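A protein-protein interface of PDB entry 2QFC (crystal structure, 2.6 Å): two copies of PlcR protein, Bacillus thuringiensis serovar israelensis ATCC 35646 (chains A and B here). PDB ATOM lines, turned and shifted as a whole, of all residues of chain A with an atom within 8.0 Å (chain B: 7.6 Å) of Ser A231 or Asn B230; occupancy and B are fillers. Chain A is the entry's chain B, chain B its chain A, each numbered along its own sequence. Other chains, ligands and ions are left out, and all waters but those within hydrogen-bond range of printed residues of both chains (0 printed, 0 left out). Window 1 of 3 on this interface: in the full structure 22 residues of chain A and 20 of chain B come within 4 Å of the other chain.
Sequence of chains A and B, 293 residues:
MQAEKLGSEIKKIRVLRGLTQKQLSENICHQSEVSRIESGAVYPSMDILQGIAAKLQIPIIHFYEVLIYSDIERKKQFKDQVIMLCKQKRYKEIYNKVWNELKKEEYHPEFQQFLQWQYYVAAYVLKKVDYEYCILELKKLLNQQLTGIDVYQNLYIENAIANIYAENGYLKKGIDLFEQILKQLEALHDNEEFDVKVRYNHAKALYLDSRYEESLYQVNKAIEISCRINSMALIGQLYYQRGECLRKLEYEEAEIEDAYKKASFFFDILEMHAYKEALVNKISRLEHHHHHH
Ser A226 touches Met B232, and with the chains exchanged Met A232 touches Ser B226. Asn A230 touches Ser B231, and with the chains exchanged Ser A231 touches Asn B230. Asn A230 touches Met B232, and with the chains exchanged Met A232 touches Asn B230. Met A232 touches Cys B227, but with the chains exchanged Cys A227 does not touch Met B232 (4.03 Å). Positions printed for both chains: 193, 225, 226, 227, 228, 229, 230, 231, 232, 233 and 270.
Among the printed residues, pairs that only touch across the chains: Met A232 with Met B232 (2.9 Å), Leu A270 with Cys B227 (3.4 Å), Cys A227 with Leu B270 (3.5 Å), Leu A270 with Asn B230 (3.6 Å), Met A232 with Ser B226 (3.6 Å), Ser A231 with Met B232 (3.7 Å), Asn A230 with Leu B270 (3.7 Å), Asn A230 with Ser B231 (3.7 Å), Asn A230 with Ala B233 (3.8 Å), Ser A231 with Asn B230 (3.8 Å), Ala A233 with Asn B230 (3.8 Å), Met A232 with Ser B231 (3.8 Å), Ile A235 with Met B232 (3.9 Å), Ser A226 with Met B232 (3.9 Å) and Met A232 with Cys B227 (3.98 Å).
Of the 12 printed residues of chain B, 7 touch a printed residue of chain A. Printed residues of chain B that touch a printed residue of chain A: Ser B226, Cys B227, Asn B230, Ser B231, Met B232, Ala B233 and Leu B270. Printed residues of chain A that touch a printed residue of chain B: Lys A87, Ser A226, Cys A227, Asn A230, Ser A231, Met A232, Ala A233, Ile A235, Ile A269 and Leu A270. Among the printed residues, no Asp or Glu carboxylate lies within 4 Å of a Lys or Arg side-chain nitrogen of the other chain.
Of the printed residues of chain B, Lys A87 touches Asn B230. Val A196 touches none of the printed residues of chain B. Ser A231 touches just these residues of chain B: Asn B230 and Met B232. Of the printed residues of chain B, Ala A233 touches Asn B230. Printed residues of chain B within 4 Å of Leu A270: Cys B227 (3.4 Å) and Asn B230 (3.6 Å). Of the printed residues of chain A, Asn B230 touches Lys A87, Ser A231, Met A232, Ala A233 and Leu A270. Of the printed residues of chain A, Ser B231 touches Asn A230 (3.7 Å) and Met A232 (3.8 Å). Printed residues of chain A within 4 Å of Met B232: Ser A226 (3.9 Å), Asn A230 (2.8 Å), Ser A231 (3.7 Å), Met A232 (2.9 Å) and Ile A235 (3.9 Å). The nearest printed residue of chain A that does not touch Ala B233 is Ser A231 (6.1 Å).
The backbone carbonyl oxygen (O) of Asn A230 lies within hydrogen-bond range of the backbone NH (N) of Met B232, at 2.8 Å. The backbone NH of Met A232 sits at hydrogen-bond distance from the backbone carbonyl oxygen of Asn B230, at 2.8 Å. The side-chain amide nitrogen (ND2) of Asn B230 sits close to the side-chain amino group (NZ) of Lys A87 (3.5 Å). SG of Cys B227 sits close to O of Ile A269 (3.5 Å).
O of Ser A226 sits at hydrogen-bond distance from N of Ser A231 (3.0 Å). O of Ser B226 lies within hydrogen-bond range of N of Ser B231, at 2.8 Å. N of Ala A233 is in hydrogen-bond range of OG of Ser A231 (2.9 Å). OD1 of Asn B230 sits close to O of Cys B227 (3.5 Å). The side-chain sulfur (SG) of Cys A227 lies within hydrogen-bond range of the backbone carbonyl oxygen (O) of Ile A223, at 3.5 Å. The side-chain hydroxyl (OG) of Ser B231 sits at hydrogen-bond distance from the backbone NH (N) of Ala B233, at 2.9 Å.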
ATOM      1  N   LYS A  87     -15.214 -27.697 -34.023  1.00  0.00           N
ATOM      2  CA  LYS A  87     -16.314 -26.762 -34.159  1.00  0.00           C
ATOM      3  C   LYS A  87     -16.455 -26.361 -35.626  1.00  0.00           C
ATOM      4  O   LYS A  87     -17.555 -26.401 -36.189  1.00  0.00           O
ATOM      5  CB  LYS A  87     -16.129 -25.575 -33.197  1.00  0.00           C
ATOM      6  CG  LYS A  87     -16.397 -24.199 -33.744  1.00  0.00           C
ATOM      7  CD  LYS A  87     -17.811 -23.711 -33.468  1.00  0.00           C
ATOM      8  CE  LYS A  87     -17.937 -22.242 -33.765  1.00  0.00           C
ATOM      9  NZ  LYS A  87     -19.264 -22.023 -34.376  1.00  0.00           N
ATOM     10  N   GLU A 192     -20.149 -26.819 -18.084  1.00  0.00           N
ATOM     11  CA  GLU A 192     -21.520 -26.823 -18.442  1.00  0.00           C
ATOM     12  C   GLU A 192     -21.690 -26.708 -19.927  1.00  0.00           C
ATOM     13  O   GLU A 192     -22.754 -27.023 -20.452  1.00  0.00           O
ATOM     14  CB  GLU A 192     -22.275 -25.768 -17.627  1.00  0.00           C
ATOM     15  CG  GLU A 192     -22.330 -26.179 -16.160  1.00  0.00           C
ATOM     16  CD  GLU A 192     -23.319 -25.384 -15.314  1.00  0.00           C
ATOM     17  OE1 GLU A 192     -22.959 -24.304 -14.771  1.00  0.00           O
ATOM     18  OE2 GLU A 192     -24.467 -25.870 -15.175  1.00  0.00           O
ATOM     19  N   GLU A 193     -20.638 -26.318 -20.626  1.00  0.00           N
ATOM     20  CA  GLU A 193     -20.733 -26.331 -22.073  1.00  0.00           C
ATOM     21  C   GLU A 193     -20.890 -27.719 -22.615  1.00  0.00           C
ATOM     22  O   GLU A 193     -21.696 -27.928 -23.479  1.00  0.00           O
ATOM     23  CB  GLU A 193     -19.601 -25.593 -22.762  1.00  0.00           C
ATOM     24  CG  GLU A 193     -20.111 -24.261 -23.348  1.00  0.00           C
ATOM     25  CD  GLU A 193     -19.021 -23.457 -24.029  1.00  0.00           C
ATOM     26  OE1 GLU A 193     -19.082 -23.355 -25.288  1.00  0.00           O
ATOM     27  OE2 GLU A 193     -18.097 -22.956 -23.299  1.00  0.00           O
ATOM     28  N   VAL A 196     -24.391 -29.055 -21.771  1.00  0.00           N
ATOM     29  CA  VAL A 196     -25.319 -28.605 -22.797  1.00  0.00           C
ATOM     30  C   VAL A 196     -25.243 -29.460 -24.037  1.00  0.00           C
ATOM     31  O   VAL A 196     -26.277 -29.782 -24.636  1.00  0.00           O
ATOM     32  CB  VAL A 196     -25.041 -27.123 -23.215  1.00  0.00           C
ATOM     33  CG1 VAL A 196     -25.703 -26.785 -24.585  1.00  0.00           C
ATOM     34  CG2 VAL A 196     -25.475 -26.142 -22.103  1.00  0.00           C
ATOM     35  N   ALA A 222     -31.485 -27.565 -21.553  1.00  0.00           N
ATOM     36  CA  ALA A 222     -30.197 -27.161 -22.138  1.00  0.00           C
ATOM     37  C   ALA A 222     -30.154 -25.661 -22.343  1.00  0.00           C
ATOM     38  O   ALA A 222     -29.148 -25.006 -22.053  1.00  0.00           O
ATOM     39  CB  ALA A 222     -29.882 -27.890 -23.385  1.00  0.00           C
ATOM     40  N   ILE A 223     -31.262 -25.124 -22.823  1.00  0.00           N
ATOM     41  CA  ILE A 223     -31.452 -23.697 -22.952  1.00  0.00           C
ATOM     42  C   ILE A 223     -31.189 -23.011 -21.613  1.00  0.00           C
ATOM     43  O   ILE A 223     -30.394 -22.052 -21.531  1.00  0.00           O
ATOM     44  CB  ILE A 223     -32.866 -23.349 -23.541  1.00  0.00           C
ATOM     45  CG1 ILE A 223     -32.980 -23.961 -24.953  1.00  0.00           C
ATOM     46  CG2 ILE A 223     -33.043 -21.823 -23.621  1.00  0.00           C
ATOM     47  CD1 ILE A 223     -34.352 -23.934 -25.641  1.00  0.00           C
ATOM     48  N   ILE A 225     -29.416 -24.004 -19.343  1.00  0.00           N
ATOM     49  CA  ILE A 225     -28.032 -24.035 -18.901  1.00  0.00           C
ATOM     50  C   ILE A 225     -27.263 -23.077 -19.751  1.00  0.00           C
ATOM     51  O   ILE A 225     -26.419 -22.336 -19.252  1.00  0.00           O
ATOM     52  CB  ILE A 225     -27.428 -25.417 -18.932  1.00  0.00           C
ATOM     53  CG1 ILE A 225     -28.050 -26.287 -17.845  1.00  0.00           C
ATOM     54  CG2 ILE A 225     -25.951 -25.334 -18.665  1.00  0.00           C
ATOM     55  CD1 ILE A 225     -27.905 -27.767 -18.131  1.00  0.00           C
ATOM     56  N   SER A 226     -27.617 -23.061 -21.029  1.00  0.00           N
ATOM     57  CA  SER A 226     -26.975 -22.237 -22.015  1.00  0.00           C
ATOM     58  C   SER A 226     -27.065 -20.794 -21.576  1.00  0.00           C
ATOM     59  O   SER A 226     -26.099 -20.045 -21.671  1.00  0.00           O
ATOM     60  CB  SER A 226     -27.725 -22.420 -23.312  1.00  0.00           C
ATOM     61  OG  SER A 226     -26.865 -22.718 -24.381  1.00  0.00           O
ATOM     62  N   CYS A 227     -28.222 -20.377 -21.078  1.00  0.00           N
ATOM     63  CA  CYS A 227     -28.364 -18.990 -20.669  1.00  0.00           C
ATOM     64  C   CYS A 227     -27.601 -18.726 -19.395  1.00  0.00           C
ATOM     65  O   CYS A 227     -27.106 -17.640 -19.177  1.00  0.00           O
ATOM     66  CB  CYS A 227     -29.817 -18.641 -20.477  1.00  0.00           C
ATOM     67  SG  CYS A 227     -30.755 -18.618 -22.014  1.00  0.00           S
ATOM     68  N   ARG A 228     -27.489 -19.701 -18.524  1.00  0.00           N
ATOM     69  CA  ARG A 228     -26.780 -19.427 -17.263  1.00  0.00           C
ATOM     70  C   ARG A 228     -25.254 -19.299 -17.457  1.00  0.00           C
ATOM     71  O   ARG A 228     -24.603 -18.636 -16.675  1.00  0.00           O
ATOM     72  CB  ARG A 228     -27.118 -20.470 -16.177  1.00  0.00           C
ATOM     73  CG  ARG A 228     -27.013 -19.898 -14.756  1.00  0.00           C
ATOM     74  CD  ARG A 228     -26.855 -20.976 -13.630  1.00  0.00           C
ATOM     75  NE  ARG A 228     -26.275 -22.269 -14.063  1.00  0.00           N
ATOM     76  CZ  ARG A 228     -27.007 -23.344 -14.350  1.00  0.00           C
ATOM     77  NH1 ARG A 228     -28.340 -23.285 -14.280  1.00  0.00           N
ATOM     78  NH2 ARG A 228     -26.421 -24.470 -14.725  1.00  0.00           N
ATOM     79  N   ILE A 229     -24.685 -19.912 -18.491  1.00  0.00           N
ATOM     80  CA  ILE A 229     -23.234 -19.794 -18.697  1.00  0.00           C
ATOM     81  C   ILE A 229     -22.940 -18.869 -19.842  1.00  0.00           C
ATOM     82  O   ILE A 229     -21.809 -18.818 -20.324  1.00  0.00           O
ATOM     83  CB  ILE A 229     -22.568 -21.128 -19.041  1.00  0.00           C
ATOM     84  CG1 ILE A 229     -23.071 -21.638 -20.397  1.00  0.00           C
ATOM     85  CG2 ILE A 229     -22.836 -22.150 -17.947  1.00  0.00           C
ATOM     86  CD1 ILE A 229     -22.184 -22.715 -21.032  1.00  0.00           C
ATOM     87  N   ASN A 230     -23.972 -18.181 -20.302  1.00  0.00           N
ATOM     88  CA  ASN A 230     -23.846 -17.184 -21.339  1.00  0.00           C
ATOM     89  C   ASN A 230     -23.347 -17.717 -22.667  1.00  0.00           C
ATOM     90  O   ASN A 230     -22.688 -16.982 -23.407  1.00  0.00           O
ATOM     91  CB  ASN A 230     -22.972 -16.018 -20.894  1.00  0.00           C
ATOM     92  CG  ASN A 230     -23.565 -15.256 -19.744  1.00  0.00           C
ATOM     93  OD1 ASN A 230     -24.759 -15.025 -19.684  1.00  0.00           O
ATOM     94  ND2 ASN A 230     -22.731 -14.857 -18.827  1.00  0.00           N
ATOM     95  N   SER A 231     -23.705 -18.949 -23.006  1.00  0.00           N
ATOM     96  CA  SER A 231     -23.256 -19.485 -24.273  1.00  0.00           C
ATOM     97  C   SER A 231     -24.260 -19.642 -25.386  1.00  0.00           C
ATOM     98  O   SER A 231     -25.327 -20.241 -25.231  1.00  0.00           O
ATOM     99  CB  SER A 231     -22.567 -20.819 -24.107  1.00  0.00           C
ATOM    100  OG  SER A 231     -22.283 -21.314 -25.405  1.00  0.00           O
ATOM    101  N   MET A 232     -23.858 -19.159 -26.553  1.00  0.00           N
ATOM    102  CA  MET A 232     -24.691 -19.274 -27.722  1.00  0.00           C
ATOM    103  C   MET A 232     -24.241 -20.437 -28.543  1.00  0.00           C
ATOM    104  O   MET A 232     -24.743 -20.619 -29.601  1.00  0.00           O
ATOM    105  CB  MET A 232     -24.619 -18.014 -28.605  1.00  0.00           C
ATOM    106  CG  MET A 232     -24.720 -16.694 -27.923  1.00  0.00           C
ATOM    107  SD  MET A 232     -25.316 -15.431 -29.057  1.00  0.00           S
ATOM    108  CE  MET A 232     -23.809 -14.642 -29.569  1.00  0.00           C
ATOM    109  N   ALA A 233     -23.274 -21.212 -28.090  1.00  0.00           N
ATOM    110  CA  ALA A 233     -22.701 -22.272 -28.959  1.00  0.00           C
ATOM    111  C   ALA A 233     -23.739 -23.145 -29.668  1.00  0.00           C
ATOM    112  O   ALA A 233     -23.667 -23.306 -30.899  1.00  0.00           O
ATOM    113  CB  ALA A 233     -21.723 -23.120 -28.207  1.00  0.00           C
ATOM    114  N   LEU A 234     -24.711 -23.640 -28.908  1.00  0.00           N
ATOM    115  CA  LEU A 234     -25.754 -24.541 -29.405  1.00  0.00           C
ATOM    116  C   LEU A 234     -27.166 -24.001 -29.293  1.00  0.00           C
ATOM    117  O   LEU A 234     -28.111 -24.699 -29.622  1.00  0.00           O
ATOM    118  CB  LEU A 234     -25.708 -25.894 -28.651  1.00  0.00           C
ATOM    119  CG  LEU A 234     -24.526 -26.767 -29.125  1.00  0.00           C
ATOM    120  CD1 LEU A 234     -24.425 -28.035 -28.370  1.00  0.00           C
ATOM    121  CD2 LEU A 234     -24.654 -27.048 -30.627  1.00  0.00           C
ATOM    122  N   ILE A 235     -27.324 -22.757 -28.864  1.00  0.00           N
ATOM    123  CA  ILE A 235     -28.665 -22.259 -28.531  1.00  0.00           C
ATOM    124  C   ILE A 235     -29.629 -22.110 -29.704  1.00  0.00           C
ATOM    125  O   ILE A 235     -30.834 -22.275 -29.538  1.00  0.00           O
ATOM    126  CB  ILE A 235     -28.612 -20.976 -27.693  1.00  0.00           C
ATOM    127  CG1 ILE A 235     -29.821 -20.911 -26.773  1.00  0.00           C
ATOM    128  CG2 ILE A 235     -28.475 -19.757 -28.561  1.00  0.00           C
ATOM    129  CD1 ILE A 235     -29.965 -19.568 -26.033  1.00  0.00           C
ATOM    130  N   GLY A 236     -29.114 -21.800 -30.886  1.00  0.00           N
ATOM    131  CA  GLY A 236     -29.957 -21.753 -32.082  1.00  0.00           C
ATOM    132  C   GLY A 236     -30.484 -23.158 -32.341  1.00  0.00           C
ATOM    133  O   GLY A 236     -31.686 -23.376 -32.552  1.00  0.00           O
ATOM    134  N   LEU A 238     -30.922 -25.426 -30.287  1.00  0.00           N
ATOM    135  CA  LEU A 238     -31.840 -25.760 -29.243  1.00  0.00           C
ATOM    136  C   LEU A 238     -33.243 -25.210 -29.520  1.00  0.00           C
ATOM    137  O   LEU A 238     -34.207 -25.958 -29.530  1.00  0.00           O
ATOM    138  CB  LEU A 238     -31.309 -25.274 -27.926  1.00  0.00           C
ATOM    139  CG  LEU A 238     -30.162 -26.198 -27.495  1.00  0.00           C
ATOM    140  CD1 LEU A 238     -29.198 -25.611 -26.494  1.00  0.00           C
ATOM    141  CD2 LEU A 238     -30.769 -27.456 -26.933  1.00  0.00           C
ATOM    142  N   PHE A 266     -30.872 -16.546 -33.934  1.00  0.00           N
ATOM    143  CA  PHE A 266     -29.524 -17.026 -33.641  1.00  0.00           C
ATOM    144  C   PHE A 266     -28.776 -17.422 -34.895  1.00  0.00           C
ATOM    145  O   PHE A 266     -27.571 -17.222 -34.991  1.00  0.00           O
ATOM    146  CB  PHE A 266     -29.488 -18.100 -32.560  1.00  0.00           C
ATOM    147  CG  PHE A 266     -29.651 -17.536 -31.182  1.00  0.00           C
ATOM    148  CD1 PHE A 266     -28.645 -16.747 -30.615  1.00  0.00           C
ATOM    149  CD2 PHE A 266     -30.834 -17.718 -30.475  1.00  0.00           C
ATOM    150  CE1 PHE A 266     -28.810 -16.174 -29.347  1.00  0.00           C
ATOM    151  CE2 PHE A 266     -31.000 -17.159 -29.208  1.00  0.00           C
ATOM    152  CZ  PHE A 266     -29.994 -16.383 -28.643  1.00  0.00           C
ATOM    153  N   ILE A 269     -27.362 -13.914 -36.705  1.00  0.00           N
ATOM    154  CA  ILE A 269     -26.354 -13.471 -35.745  1.00  0.00           C
ATOM    155  C   ILE A 269     -25.062 -14.306 -35.808  1.00  0.00           C
ATOM    156  O   ILE A 269     -23.969 -13.740 -35.817  1.00  0.00           O
ATOM    157  CB  ILE A 269     -26.956 -13.601 -34.345  1.00  0.00           C
ATOM    158  CG1 ILE A 269     -27.367 -12.266 -33.764  1.00  0.00           C
ATOM    159  CG2 ILE A 269     -26.012 -14.216 -33.396  1.00  0.00           C
ATOM    160  CD1 ILE A 269     -27.499 -12.430 -32.253  1.00  0.00           C
ATOM    161  N   LEU A 270     -25.187 -15.638 -35.866  1.00  0.00           N
ATOM    162  CA  LEU A 270     -24.026 -16.513 -35.819  1.00  0.00           C
ATOM    163  C   LEU A 270     -23.694 -16.898 -37.239  1.00  0.00           C
ATOM    164  O   LEU A 270     -22.781 -17.688 -37.500  1.00  0.00           O
ATOM    165  CB  LEU A 270     -24.268 -17.735 -34.929  1.00  0.00           C
ATOM    166  CG  LEU A 270     -24.695 -17.288 -33.518  1.00  0.00           C
ATOM    167  CD1 LEU A 270     -25.249 -18.359 -32.575  1.00  0.00           C
ATOM    168  CD2 LEU A 270     -23.573 -16.544 -32.825  1.00  0.00           C
ATOM    169  N   GLU A 271     -24.437 -16.308 -38.171  1.00  0.00           N
ATOM    170  CA  GLU A 271     -24.213 -16.514 -39.599  1.00  0.00           C
ATOM    171  C   GLU A 271     -24.044 -18.003 -39.911  1.00  0.00           C
ATOM    172  O   GLU A 271     -23.205 -18.410 -40.726  1.00  0.00           O
ATOM    173  CB  GLU A 271     -23.044 -15.668 -40.073  1.00  0.00           C
ATOM    174  CG  GLU A 271     -23.421 -14.211 -40.245  1.00  0.00           C
ATOM    175  CD  GLU A 271     -22.216 -13.303 -40.218  1.00  0.00           C
ATOM    176  OE1 GLU A 271     -21.102 -13.845 -40.064  1.00  0.00           O
ATOM    177  OE2 GLU A 271     -22.371 -12.061 -40.356  1.00  0.00           O
ATOM    178  N   MET A 272     -24.859 -18.803 -39.226  1.00  0.00           N
ATOM    179  CA  MET A 272     -24.861 -20.235 -39.406  1.00  0.00           C
ATOM    180  C   MET A 272     -25.708 -20.531 -40.629  1.00  0.00           C
ATOM    181  O   MET A 272     -26.877 -20.921 -40.521  1.00  0.00           O
ATOM    182  CB  MET A 272     -25.419 -20.916 -38.160  1.00  0.00           C
ATOM    183  CG  MET A 272     -24.440 -20.943 -37.003  1.00  0.00           C
ATOM    184  SD  MET A 272     -25.327 -21.411 -35.511  1.00  0.00           S
ATOM    185  CE  MET A 272     -24.002 -21.274 -34.297  1.00  0.00           C
ATOM    186  N   GLU B 193     -13.049 -12.872 -25.256  1.00  0.00           N
ATOM    187  CA  GLU B 193     -14.044 -12.377 -24.319  1.00  0.00           C
ATOM    188  C   GLU B 193     -13.598 -11.079 -23.731  1.00  0.00           C
ATOM    189  O   GLU B 193     -14.376 -10.148 -23.601  1.00  0.00           O
ATOM    190  CB  GLU B 193     -14.326 -13.348 -23.204  1.00  0.00           C
ATOM    191  CG  GLU B 193     -15.280 -14.447 -23.608  1.00  0.00           C
ATOM    192  CD  GLU B 193     -15.076 -15.669 -22.725  1.00  0.00           C
ATOM    193  OE1 GLU B 193     -14.938 -15.454 -21.481  1.00  0.00           O
ATOM    194  OE2 GLU B 193     -15.021 -16.814 -23.265  1.00  0.00           O
ATOM    195  N   GLU B 224     -19.924  -8.120 -33.188  1.00  0.00           N
ATOM    196  CA  GLU B 224     -19.395  -9.018 -34.180  1.00  0.00           C
ATOM    197  C   GLU B 224     -18.507 -10.058 -33.522  1.00  0.00           C
ATOM    198  O   GLU B 224     -18.541 -11.207 -33.889  1.00  0.00           O
ATOM    199  CB  GLU B 224     -18.611  -8.252 -35.228  1.00  0.00           C
ATOM    200  CG  GLU B 224     -18.510  -8.978 -36.540  1.00  0.00           C
ATOM    201  CD  GLU B 224     -17.203  -8.725 -37.264  1.00  0.00           C
ATOM    202  OE1 GLU B 224     -16.767  -7.553 -37.349  1.00  0.00           O
ATOM    203  OE2 GLU B 224     -16.619  -9.720 -37.769  1.00  0.00           O
ATOM    204  N   ILE B 225     -17.731  -9.672 -32.524  1.00  0.00           N
ATOM    205  CA  ILE B 225     -16.781 -10.624 -31.919  1.00  0.00           C
ATOM    206  C   ILE B 225     -17.520 -11.582 -31.002  1.00  0.00           C
ATOM    207  O   ILE B 225     -17.263 -12.813 -31.034  1.00  0.00           O
ATOM    208  CB  ILE B 225     -15.651  -9.917 -31.189  1.00  0.00           C
ATOM    209  CG1 ILE B 225     -14.707  -9.257 -32.186  1.00  0.00           C
ATOM    210  CG2 ILE B 225     -14.796 -10.899 -30.386  1.00  0.00           C
ATOM    211  CD1 ILE B 225     -13.850  -8.179 -31.546  1.00  0.00           C
ATOM    212  N   SER B 226     -18.464 -11.027 -30.236  1.00  0.00           N
ATOM    213  CA  SER B 226     -19.346 -11.795 -29.401  1.00  0.00           C
ATOM    214  C   SER B 226     -20.013 -12.900 -30.174  1.00  0.00           C
ATOM    215  O   SER B 226     -20.238 -13.996 -29.633  1.00  0.00           O
ATOM    216  CB  SER B 226     -20.428 -10.899 -28.841  1.00  0.00           C
ATOM    217  OG  SER B 226     -20.203 -10.598 -27.484  1.00  0.00           O
ATOM    218  N   CYS B 227     -20.357 -12.644 -31.433  1.00  0.00           N
ATOM    219  CA  CYS B 227     -21.003 -13.677 -32.215  1.00  0.00           C
ATOM    220  C   CYS B 227     -19.989 -14.694 -32.724  1.00  0.00           C
ATOM    221  O   CYS B 227     -20.296 -15.846 -32.934  1.00  0.00           O
ATOM    222  CB  CYS B 227     -21.772 -13.056 -33.363  1.00  0.00           C
ATOM    223  SG  CYS B 227     -23.254 -12.067 -32.839  1.00  0.00           S
ATOM    224  N   ARG B 228     -18.754 -14.307 -32.923  1.00  0.00           N
ATOM    225  CA  ARG B 228     -17.846 -15.253 -33.561  1.00  0.00           C
ATOM    226  C   ARG B 228     -17.298 -16.248 -32.515  1.00  0.00           C
ATOM    227  O   ARG B 228     -16.981 -17.369 -32.853  1.00  0.00           O
ATOM    228  CB  ARG B 228     -16.731 -14.491 -34.301  1.00  0.00           C
ATOM    229  CG  ARG B 228     -15.908 -15.319 -35.280  1.00  0.00           C
ATOM    230  CD  ARG B 228     -15.006 -14.479 -36.255  1.00  0.00           C
ATOM    231  NE  ARG B 228     -14.763 -13.078 -35.857  1.00  0.00           N
ATOM    232  CZ  ARG B 228     -13.894 -12.685 -34.921  1.00  0.00           C
ATOM    233  NH1 ARG B 228     -13.177 -13.586 -34.248  1.00  0.00           N
ATOM    234  NH2 ARG B 228     -13.751 -11.383 -34.651  1.00  0.00           N
ATOM    235  N   ILE B 229     -17.223 -15.834 -31.241  1.00  0.00           N
ATOM    236  CA  ILE B 229     -16.753 -16.729 -30.167  1.00  0.00           C
ATOM    237  C   ILE B 229     -17.928 -17.347 -29.435  1.00  0.00           C
ATOM    238  O   ILE B 229     -17.733 -18.044 -28.461  1.00  0.00           O
ATOM    239  CB  ILE B 229     -15.835 -16.006 -29.158  1.00  0.00           C
ATOM    240  CG1 ILE B 229     -16.613 -14.950 -28.353  1.00  0.00           C
ATOM    241  CG2 ILE B 229     -14.705 -15.334 -29.894  1.00  0.00           C
ATOM    242  CD1 ILE B 229     -15.738 -14.067 -27.438  1.00  0.00           C
ATOM    243  N   ASN B 230     -19.140 -17.038 -29.892  1.00  0.00           N
ATOM    244  CA  ASN B 230     -20.366 -17.604 -29.358  1.00  0.00           C
ATOM    245  C   ASN B 230     -20.772 -17.138 -27.952  1.00  0.00           C
ATOM    246  O   ASN B 230     -21.434 -17.878 -27.199  1.00  0.00           O
ATOM    247  CB  ASN B 230     -20.400 -19.145 -29.479  1.00  0.00           C
ATOM    248  CG  ASN B 230     -20.509 -19.619 -30.928  1.00  0.00           C
ATOM    249  OD1 ASN B 230     -21.165 -19.003 -31.757  1.00  0.00           O
ATOM    250  ND2 ASN B 230     -19.863 -20.708 -31.231  1.00  0.00           N
ATOM    251  N   SER B 231     -20.492 -15.888 -27.622  1.00  0.00           N
ATOM    252  CA  SER B 231     -20.729 -15.488 -26.255  1.00  0.00           C
ATOM    253  C   SER B 231     -21.778 -14.456 -26.009  1.00  0.00           C
ATOM    254  O   SER B 231     -21.742 -13.384 -26.583  1.00  0.00           O
ATOM    255  CB  SER B 231     -19.447 -15.031 -25.580  1.00  0.00           C
ATOM    256  OG  SER B 231     -19.821 -14.414 -24.368  1.00  0.00           O
ATOM    257  N   MET B 232     -22.679 -14.756 -25.083  1.00  0.00           N
ATOM    258  CA  MET B 232     -23.737 -13.821 -24.736  1.00  0.00           C
ATOM    259  C   MET B 232     -23.346 -12.996 -23.531  1.00  0.00           C
ATOM    260  O   MET B 232     -24.206 -12.347 -22.973  1.00  0.00           O
ATOM    261  CB  MET B 232     -25.033 -14.569 -24.380  1.00  0.00           C
ATOM    262  CG  MET B 232     -25.467 -15.619 -25.324  1.00  0.00           C
ATOM    263  SD  MET B 232     -27.262 -15.837 -25.211  1.00  0.00           S
ATOM    264  CE  MET B 232     -27.388 -17.350 -24.214  1.00  0.00           C
ATOM    265  N   ALA B 233     -22.093 -13.057 -23.082  1.00  0.00           N
ATOM    266  CA  ALA B 233     -21.708 -12.417 -21.808  1.00  0.00           C
ATOM    267  C   ALA B 233     -22.072 -10.914 -21.696  1.00  0.00           C
ATOM    268  O   ALA B 233     -22.572 -10.474 -20.653  1.00  0.00           O
ATOM    269  CB  ALA B 233     -20.218 -12.636 -21.508  1.00  0.00           C
ATOM    270  N   LEU B 270     -31.434 -13.880 -20.356  1.00  0.00           N
ATOM    271  CA  LEU B 270     -30.392 -13.967 -19.335  1.00  0.00           C
ATOM    272  C   LEU B 270     -30.854 -13.676 -17.918  1.00  0.00           C
ATOM    273  O   LEU B 270     -30.045 -13.664 -17.005  1.00  0.00           O
ATOM    274  CB  LEU B 270     -29.168 -13.114 -19.675  1.00  0.00           C
ATOM    275  CG  LEU B 270     -28.506 -13.456 -21.002  1.00  0.00           C
ATOM    276  CD1 LEU B 270     -27.209 -12.707 -21.250  1.00  0.00           C
ATOM    277  CD2 LEU B 270     -28.306 -14.974 -21.093  1.00  0.00           C
